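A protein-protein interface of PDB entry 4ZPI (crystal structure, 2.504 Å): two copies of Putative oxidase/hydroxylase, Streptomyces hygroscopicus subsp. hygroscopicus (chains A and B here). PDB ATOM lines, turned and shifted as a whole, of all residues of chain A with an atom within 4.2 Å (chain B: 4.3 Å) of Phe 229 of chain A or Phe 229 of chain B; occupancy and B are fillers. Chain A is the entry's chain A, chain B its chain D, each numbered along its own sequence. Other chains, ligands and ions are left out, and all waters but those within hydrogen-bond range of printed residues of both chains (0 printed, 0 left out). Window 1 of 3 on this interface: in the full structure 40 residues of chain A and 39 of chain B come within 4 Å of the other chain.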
ATOM      1  N   ARG A  84       1.729  19.576   2.990  1.00  0.00           N
ATOM      2  CA  ARG A  84       0.616  19.010   3.750  1.00  0.00           C
ATOM      3  C   ARG A  84      -0.243  18.092   2.881  1.00  0.00           C
ATOM      4  O   ARG A  84      -0.554  18.448   1.746  1.00  0.00           O
ATOM      5  CB  ARG A  84      -0.254  20.125   4.336  1.00  0.00           C
ATOM      6  CG  ARG A  84      -1.478  19.613   5.059  1.00  0.00           C
ATOM      7  CD  ARG A  84      -2.314  20.717   5.691  1.00  0.00           C
ATOM      8  NE  ARG A  84      -3.296  20.131   6.599  1.00  0.00           N
ATOM      9  CZ  ARG A  84      -4.372  20.750   7.071  1.00  0.00           C
ATOM     10  NH1 ARG A  84      -4.645  22.002   6.734  1.00  0.00           N
ATOM     11  NH2 ARG A  84      -5.184  20.107   7.887  1.00  0.00           N
ATOM     12  N   LEU A  86      -3.611  16.893   1.624  1.00  0.00           N
ATOM     13  CA  LEU A  86      -4.871  17.616   1.590  1.00  0.00           C
ATOM     14  C   LEU A  86      -6.055  16.697   1.255  1.00  0.00           C
ATOM     15  O   LEU A  86      -7.205  17.023   1.559  1.00  0.00           O
ATOM     16  CB  LEU A  86      -4.779  18.778   0.585  1.00  0.00           C
ATOM     17  CG  LEU A  86      -3.850  19.952   0.957  1.00  0.00           C
ATOM     18  CD1 LEU A  86      -3.814  21.050  -0.121  1.00  0.00           C
ATOM     19  CD2 LEU A  86      -4.210  20.566   2.307  1.00  0.00           C
ATOM     20  N   SER A 121      -6.295  28.831  -5.338  1.00  0.00           N
ATOM     21  CA  SER A 121      -5.928  27.485  -4.913  1.00  0.00           C
ATOM     22  C   SER A 121      -5.210  26.735  -6.011  1.00  0.00           C
ATOM     23  O   SER A 121      -4.733  25.642  -5.782  1.00  0.00           O
ATOM     24  CB  SER A 121      -7.153  26.687  -4.484  1.00  0.00           C
ATOM     25  OG  SER A 121      -8.134  26.708  -5.504  1.00  0.00           O
ATOM     26  N   PRO A 134       0.486  25.478  -5.962  1.00  0.00           N
ATOM     27  CA  PRO A 134      -0.089  25.291  -4.631  1.00  0.00           C
ATOM     28  C   PRO A 134      -0.938  24.005  -4.470  1.00  0.00           C
ATOM     29  O   PRO A 134      -1.148  23.560  -3.346  1.00  0.00           O
ATOM     30  CB  PRO A 134      -0.948  26.533  -4.473  1.00  0.00           C
ATOM     31  CG  PRO A 134      -1.381  26.845  -5.881  1.00  0.00           C
ATOM     32  CD  PRO A 134      -0.218  26.514  -6.738  1.00  0.00           C
ATOM     33  N   PRO A 226       0.462  23.474   0.302  1.00  0.00           N
ATOM     34  CA  PRO A 226       1.130  24.145   1.418  1.00  0.00           C
ATOM     35  C   PRO A 226       0.447  23.836   2.738  1.00  0.00           C
ATOM     36  O   PRO A 226      -0.732  23.504   2.729  1.00  0.00           O
ATOM     37  CB  PRO A 226       0.993  25.637   1.062  1.00  0.00           C
ATOM     38  CG  PRO A 226       0.747  25.664  -0.403  1.00  0.00           C
ATOM     39  CD  PRO A 226      -0.040  24.436  -0.695  1.00  0.00           C
ATOM     40  N   THR A 227       1.156  23.985   3.849  1.00  0.00           N
ATOM     41  CA  THR A 227       0.598  23.645   5.159  1.00  0.00           C
ATOM     42  C   THR A 227      -0.525  24.586   5.615  1.00  0.00           C
ATOM     43  O   THR A 227      -1.195  24.315   6.622  1.00  0.00           O
ATOM     44  CB  THR A 227       1.693  23.637   6.227  1.00  0.00           C
ATOM     45  OG1 THR A 227       2.301  24.930   6.294  1.00  0.00           O
ATOM     46  CG2 THR A 227       2.760  22.626   5.861  1.00  0.00           C
ATOM     47  N   PHE A 228      -0.742  25.680   4.881  1.00  0.00           N
ATOM     48  CA  PHE A 228      -1.817  26.616   5.232  1.00  0.00           C
ATOM     49  C   PHE A 228      -3.081  26.443   4.374  1.00  0.00           C
ATOM     50  O   PHE A 228      -4.047  27.202   4.508  1.00  0.00           O
ATOM     51  CB  PHE A 228      -1.318  28.074   5.162  1.00  0.00           C
ATOM     52  CG  PHE A 228      -0.627  28.424   3.884  1.00  0.00           C
ATOM     53  CD1 PHE A 228       0.751  28.370   3.794  1.00  0.00           C
ATOM     54  CD2 PHE A 228      -1.354  28.828   2.770  1.00  0.00           C
ATOM     55  CE1 PHE A 228       1.402  28.703   2.611  1.00  0.00           C
ATOM     56  CE2 PHE A 228      -0.712  29.164   1.583  1.00  0.00           C
ATOM     57  CZ  PHE A 228       0.669  29.085   1.499  1.00  0.00           C
ATOM     58  N   PHE A 229      -3.079  25.452   3.493  1.00  0.00           N
ATOM     59  CA  PHE A 229      -4.314  25.077   2.816  1.00  0.00           C
ATOM     60  C   PHE A 229      -5.125  24.196   3.773  1.00  0.00           C
ATOM     61  O   PHE A 229      -4.541  23.448   4.540  1.00  0.00           O
ATOM     62  CB  PHE A 229      -4.025  24.336   1.500  1.00  0.00           C
ATOM     63  CG  PHE A 229      -3.777  25.242   0.326  1.00  0.00           C
ATOM     64  CD1 PHE A 229      -3.331  26.543   0.507  1.00  0.00           C
ATOM     65  CD2 PHE A 229      -4.015  24.802  -0.966  1.00  0.00           C
ATOM     66  CE1 PHE A 229      -3.108  27.379  -0.584  1.00  0.00           C
ATOM     67  CE2 PHE A 229      -3.796  25.628  -2.053  1.00  0.00           C
ATOM     68  CZ  PHE A 229      -3.343  26.927  -1.861  1.00  0.00           C
ATOM     69  N   THR A 230      -6.453  24.300   3.766  1.00  0.00           N
ATOM     70  CA  THR A 230      -7.279  23.361   4.537  1.00  0.00           C
ATOM     71  C   THR A 230      -7.383  22.067   3.778  1.00  0.00           C
ATOM     72  O   THR A 230      -7.239  22.068   2.555  1.00  0.00           O
ATOM     73  CB  THR A 230      -8.709  23.850   4.782  1.00  0.00           C
ATOM     74  OG1 THR A 230      -9.298  24.242   3.531  1.00  0.00           O
ATOM     75  CG2 THR A 230      -8.741  24.997   5.767  1.00  0.00           C
ATOM     76  N   GLU A 231      -7.658  20.977   4.488  1.00  0.00           N
ATOM     77  CA  GLU A 231      -7.918  19.696   3.827  1.00  0.00           C
ATOM     78  C   GLU A 231      -9.106  19.872   2.900  1.00  0.00           C
ATOM     79  O   GLU A 231      -9.991  20.688   3.175  1.00  0.00           O
ATOM     80  CB  GLU A 231      -8.171  18.573   4.838  1.00  0.00           C
ATOM     81  CG  GLU A 231      -6.924  18.153   5.616  1.00  0.00           C
ATOM     82  CD  GLU A 231      -7.238  17.209   6.765  1.00  0.00           C
ATOM     83  OE1 GLU A 231      -8.425  16.808   6.892  1.00  0.00           O
ATOM     84  OE2 GLU A 231      -6.302  16.869   7.535  1.00  0.00           O
ATOM     85  N   TYR A 247     -13.259  24.655  -0.669  1.00  0.00           N
ATOM     86  CA  TYR A 247     -12.903  25.074  -2.019  1.00  0.00           C
ATOM     87  C   TYR A 247     -14.135  25.309  -2.891  1.00  0.00           C
ATOM     88  O   TYR A 247     -14.973  24.436  -3.060  1.00  0.00           O
ATOM     89  CB  TYR A 247     -11.982  24.036  -2.666  1.00  0.00           C
ATOM     90  CG  TYR A 247     -10.670  23.799  -1.936  1.00  0.00           C
ATOM     91  CD1 TYR A 247     -10.648  23.242  -0.661  1.00  0.00           C
ATOM     92  CD2 TYR A 247      -9.449  24.107  -2.539  1.00  0.00           C
ATOM     93  CE1 TYR A 247      -9.466  23.019   0.002  1.00  0.00           C
ATOM     94  CE2 TYR A 247      -8.259  23.881  -1.887  1.00  0.00           C
ATOM     95  CZ  TYR A 247      -8.271  23.332  -0.614  1.00  0.00           C
ATOM     96  OH  TYR A 247      -7.092  23.096   0.056  1.00  0.00           O
ATOM     97  N   ARG B  84     -12.845  34.301   3.907  1.00  0.00           N
ATOM     98  CA  ARG B  84     -12.881  33.651   5.215  1.00  0.00           C
ATOM     99  C   ARG B  84     -12.115  34.506   6.224  1.00  0.00           C
ATOM    100  O   ARG B  84     -11.080  35.093   5.888  1.00  0.00           O
ATOM    101  CB  ARG B  84     -12.287  32.236   5.154  1.00  0.00           C
ATOM    102  CG  ARG B  84     -12.394  31.485   6.478  1.00  0.00           C
ATOM    103  CD  ARG B  84     -11.670  30.135   6.483  1.00  0.00           C
ATOM    104  NE  ARG B  84     -11.913  29.415   7.738  1.00  0.00           N
ATOM    105  CZ  ARG B  84     -11.305  28.288   8.120  1.00  0.00           C
ATOM    106  NH1 ARG B  84     -10.390  27.711   7.351  1.00  0.00           N
ATOM    107  NH2 ARG B  84     -11.613  27.731   9.282  1.00  0.00           N
ATOM    108  N   LEU B  86      -9.621  34.817   9.065  1.00  0.00           N
ATOM    109  CA  LEU B  86      -8.543  33.916   9.475  1.00  0.00           C
ATOM    110  C   LEU B  86      -7.956  34.229  10.843  1.00  0.00           C
ATOM    111  O   LEU B  86      -7.361  33.354  11.466  1.00  0.00           O
ATOM    112  CB  LEU B  86      -7.417  33.925   8.429  1.00  0.00           C
ATOM    113  CG  LEU B  86      -7.829  33.674   6.976  1.00  0.00           C
ATOM    114  CD1 LEU B  86      -6.648  33.823   6.053  1.00  0.00           C
ATOM    115  CD2 LEU B  86      -8.481  32.301   6.796  1.00  0.00           C
ATOM    116  N   SER B 121       1.369  31.952   0.761  1.00  0.00           N
ATOM    117  CA  SER B 121       0.330  32.562   1.592  1.00  0.00           C
ATOM    118  C   SER B 121       0.252  34.075   1.392  1.00  0.00           C
ATOM    119  O   SER B 121      -0.692  34.715   1.858  1.00  0.00           O
ATOM    120  CB  SER B 121       0.554  32.254   3.077  1.00  0.00           C
ATOM    121  OG  SER B 121       1.758  32.825   3.555  1.00  0.00           O
ATOM    122  N   PRO B 134      -4.001  37.013  -1.447  1.00  0.00           N
ATOM    123  CA  PRO B 134      -4.539  35.932  -0.629  1.00  0.00           C
ATOM    124  C   PRO B 134      -4.505  36.195   0.880  1.00  0.00           C
ATOM    125  O   PRO B 134      -5.207  35.496   1.590  1.00  0.00           O
ATOM    126  CB  PRO B 134      -3.638  34.758  -0.996  1.00  0.00           C
ATOM    127  CG  PRO B 134      -2.332  35.406  -1.325  1.00  0.00           C
ATOM    128  CD  PRO B 134      -2.630  36.741  -1.909  1.00  0.00           C
ATOM    129  N   TYR B 135      -3.721  37.146   1.382  1.00  0.00           N
ATOM    130  CA  TYR B 135      -3.752  37.391   2.822  1.00  0.00           C
ATOM    131  C   TYR B 135      -3.638  38.882   3.126  1.00  0.00           C
ATOM    132  O   TYR B 135      -2.566  39.453   3.010  1.00  0.00           O
ATOM    133  CB  TYR B 135      -2.641  36.613   3.542  1.00  0.00           C
ATOM    134  CG  TYR B 135      -2.925  36.397   5.012  1.00  0.00           C
ATOM    135  CD1 TYR B 135      -2.921  37.458   5.905  1.00  0.00           C
ATOM    136  CD2 TYR B 135      -3.223  35.127   5.510  1.00  0.00           C
ATOM    137  CE1 TYR B 135      -3.202  37.270   7.247  1.00  0.00           C
ATOM    138  CE2 TYR B 135      -3.506  34.926   6.852  1.00  0.00           C
ATOM    139  CZ  TYR B 135      -3.496  36.011   7.713  1.00  0.00           C
ATOM    140  OH  TYR B 135      -3.780  35.831   9.049  1.00  0.00           O
ATOM    141  N   PRO B 226      -8.754  33.614   1.308  1.00  0.00           N
ATOM    142  CA  PRO B 226      -9.690  32.697   0.655  1.00  0.00           C
ATOM    143  C   PRO B 226     -10.127  31.595   1.608  1.00  0.00           C
ATOM    144  O   PRO B 226      -9.416  31.321   2.579  1.00  0.00           O
ATOM    145  CB  PRO B 226      -8.876  32.124  -0.508  1.00  0.00           C
ATOM    146  CG  PRO B 226      -7.671  33.055  -0.655  1.00  0.00           C
ATOM    147  CD  PRO B 226      -7.401  33.501   0.746  1.00  0.00           C
ATOM    148  N   THR B 227     -11.277  30.985   1.324  1.00  0.00           N
ATOM    149  CA  THR B 227     -11.888  29.972   2.192  1.00  0.00           C
ATOM    150  C   THR B 227     -11.053  28.713   2.352  1.00  0.00           C
ATOM    151  O   THR B 227     -11.262  27.972   3.300  1.00  0.00           O
ATOM    152  CB  THR B 227     -13.288  29.530   1.674  1.00  0.00           C
ATOM    153  OG1 THR B 227     -13.208  29.228   0.278  1.00  0.00           O
ATOM    154  CG2 THR B 227     -14.332  30.613   1.898  1.00  0.00           C
ATOM    155  N   PHE B 228     -10.128  28.454   1.429  1.00  0.00           N
ATOM    156  CA  PHE B 228      -9.299  27.253   1.520  1.00  0.00           C
ATOM    157  C   PHE B 228      -8.026  27.472   2.329  1.00  0.00           C
ATOM    158  O   PHE B 228      -7.174  26.587   2.403  1.00  0.00           O
ATOM    159  CB  PHE B 228      -8.949  26.712   0.126  1.00  0.00           C
ATOM    160  CG  PHE B 228      -8.449  27.750  -0.834  1.00  0.00           C
ATOM    161  CD1 PHE B 228      -7.096  28.100  -0.864  1.00  0.00           C
ATOM    162  CD2 PHE B 228      -9.324  28.360  -1.731  1.00  0.00           C
ATOM    163  CE1 PHE B 228      -6.629  29.054  -1.765  1.00  0.00           C
ATOM    164  CE2 PHE B 228      -8.868  29.320  -2.636  1.00  0.00           C
ATOM    165  CZ  PHE B 228      -7.515  29.671  -2.652  1.00  0.00           C
ATOM    166  N   PHE B 229      -7.900  28.643   2.940  1.00  0.00           N
ATOM    167  CA  PHE B 229      -6.825  28.886   3.888  1.00  0.00           C
ATOM    168  C   PHE B 229      -7.244  28.429   5.273  1.00  0.00           C
ATOM    169  O   PHE B 229      -8.376  28.634   5.696  1.00  0.00           O
ATOM    170  CB  PHE B 229      -6.441  30.376   3.943  1.00  0.00           C
ATOM    171  CG  PHE B 229      -5.414  30.791   2.923  1.00  0.00           C
ATOM    172  CD1 PHE B 229      -5.330  30.156   1.685  1.00  0.00           C
ATOM    173  CD2 PHE B 229      -4.525  31.811   3.212  1.00  0.00           C
ATOM    174  CE1 PHE B 229      -4.375  30.555   0.743  1.00  0.00           C
ATOM    175  CE2 PHE B 229      -3.569  32.215   2.284  1.00  0.00           C
ATOM    176  CZ  PHE B 229      -3.496  31.586   1.050  1.00  0.00           C
ATOM    177  N   THR B 230      -6.324  27.820   5.991  1.00  0.00           N
ATOM    178  CA  THR B 230      -6.572  27.485   7.381  1.00  0.00           C
ATOM    179  C   THR B 230      -6.513  28.770   8.220  1.00  0.00           C
ATOM    180  O   THR B 230      -5.850  29.733   7.837  1.00  0.00           O
ATOM    181  CB  THR B 230      -5.546  26.443   7.889  1.00  0.00           C
ATOM    182  OG1 THR B 230      -6.095  25.724   9.000  1.00  0.00           O
ATOM    183  CG2 THR B 230      -4.237  27.114   8.298  1.00  0.00           C
ATOM    184  N   GLU B 231      -7.221  28.796   9.346  1.00  0.00           N
ATOM    185  CA  GLU B 231      -7.117  29.924  10.276  1.00  0.00           C
ATOM    186  C   GLU B 231      -5.681  30.077  10.744  1.00  0.00           C
ATOM    187  O   GLU B 231      -4.954  29.086  10.850  1.00  0.00           O
ATOM    188  CB  GLU B 231      -8.032  29.743  11.483  1.00  0.00           C
ATOM    189  CG  GLU B 231      -9.490  29.975  11.187  1.00  0.00           C
ATOM    190  CD  GLU B 231     -10.379  29.561  12.349  1.00  0.00           C
ATOM    191  OE1 GLU B 231     -11.613  29.765  12.236  1.00  0.00           O
ATOM    192  OE2 GLU B 231      -9.844  29.025  13.361  1.00  0.00           O
ATOM    193  N   TYR B 247       1.198  28.239   9.202  1.00  0.00           N
ATOM    194  CA  TYR B 247       1.973  29.134   8.361  1.00  0.00           C
ATOM    195  C   TYR B 247       3.415  29.156   8.826  1.00  0.00           C
ATOM    196  O   TYR B 247       3.696  29.510   9.961  1.00  0.00           O
ATOM    197  CB  TYR B 247       1.376  30.545   8.390  1.00  0.00           C
ATOM    198  CG  TYR B 247      -0.041  30.663   7.855  1.00  0.00           C
ATOM    199  CD1 TYR B 247      -0.296  31.245   6.622  1.00  0.00           C
ATOM    200  CD2 TYR B 247      -1.128  30.194   8.593  1.00  0.00           C
ATOM    201  CE1 TYR B 247      -1.587  31.364   6.137  1.00  0.00           C
ATOM    202  CE2 TYR B 247      -2.416  30.309   8.120  1.00  0.00           C
ATOM    203  CZ  TYR B 247      -2.647  30.887   6.891  1.00  0.00           C
ATOM    204  OH  TYR B 247      -3.945  30.993   6.428  1.00  0.00           O
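Of chain B, only Phe 228 and Phe 229 come within 4 Å of Phe 229 of chain A.
Printed residues of chain B within 4 Å of Ser 121 of chain A: Phe 228 (3.1 Å).
Of the printed residues of chain A, Thr 230 of chain B touches Phe 228 (2.8 Å) and Thr 230 (3.7 Å).
Printed residues of chain A within 4 Å of Phe 228 of chain B: Ser 121 (3.1 Å), Phe 228 (3.8 Å), Phe 229 (3.3 Å), Thr 230 (2.8 Å) and Tyr 247 (3.5 Å).
Of the printed residues of chain B, Phe 228 of chain A touches Ser 121, Phe 228, Phe 229, Thr 230 and Tyr 247.
Printed residues of chain B within 4 Å of Tyr 247 of chain A: Phe 228.
Glu 231 of chain B touches none of the printed residues of chain A.
Thr 227 of chain A touches none of the printed residues of chain B.
Phe 228 of chain A touches Phe 229 of chain B, and with the chains exchanged Phe 229 of chain A touches Phe 228 of chain B.
Phe 228 of chain A touches Tyr 247 of chain B, and with the chains exchanged Tyr 247 of chain A touches Phe 228 of chain B.
Phe 229 of chain A touches its own counterpart, Phe 229 of chain B.
Thr 230 of chain A touches its own counterpart, Thr 230 of chain B.
N of Thr 230 of chain A is in hydrogen-bond range of O of Phe 228 of chain B, at 2.8 Å.
The backbone carbonyl oxygen of Phe 228 of chain A is in hydrogen-bond range of the backbone NH of Thr 230 of chain B, at 2.8 Å.
Among the printed residues, merely in contact across the chains: Ser 121 of chain A with Phe 228 of chain B (3.1 Å), Phe 228 of chain A with Ser 121 of chain B (3.0 Å), Phe 228 of chain A with Phe 228 of chain B (3.8 Å), Phe 228 of chain A with Phe 229 of chain B (3.3 Å), Phe 228 of chain A with Tyr 247 of chain B (3.4 Å), Phe 229 of chain A with Phe 228 of chain B (3.3 Å), Phe 229 of chain A with Phe 229 of chain B (3.7 Å), Thr 230 of chain A with Arg 84 of chain B (3.5 Å), Thr 230 of chain A with Phe 229 of chain B (3.7 Å), Thr 230 of chain A with Thr 230 of chain B (3.7 Å) and Tyr 247 of chain A with Phe 228 of chain B (3.5 Å).
NH1 of Arg 84 of chain B lies within hydrogen-bond range of O of Phe 229 of chain B (2.8 Å).
The side-chain hydroxyl of Tyr 247 of chain A sits at hydrogen-bond distance from the backbone carbonyl oxygen of Thr 230 of chain A, at 2.7 Å.
The side-chain hydroxyl of Tyr 247 of chain B sits at hydrogen-bond distance from the backbone carbonyl oxygen of Thr 230 of chain B (2.7 Å).
O of Phe 229 of chain A sits at hydrogen-bond distance from NH1 of Arg 84 of chain A.
OE1 of Glu 231 of chain B is in salt-bridge range of NH2 of Arg 84 of chain B (3.6 Å).
Of the 11 printed residues of chain A, 5 touch a printed residue of chain B.
Printed residues of chain A that touch a printed residue of chain B: Ser 121, Phe 228, Phe 229, Thr 230 and Tyr 247.
Among the printed residues, no Asp or Glu carboxylate lies within 4 Å of a Lys or Arg side-chain nitrogen of the other chain.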
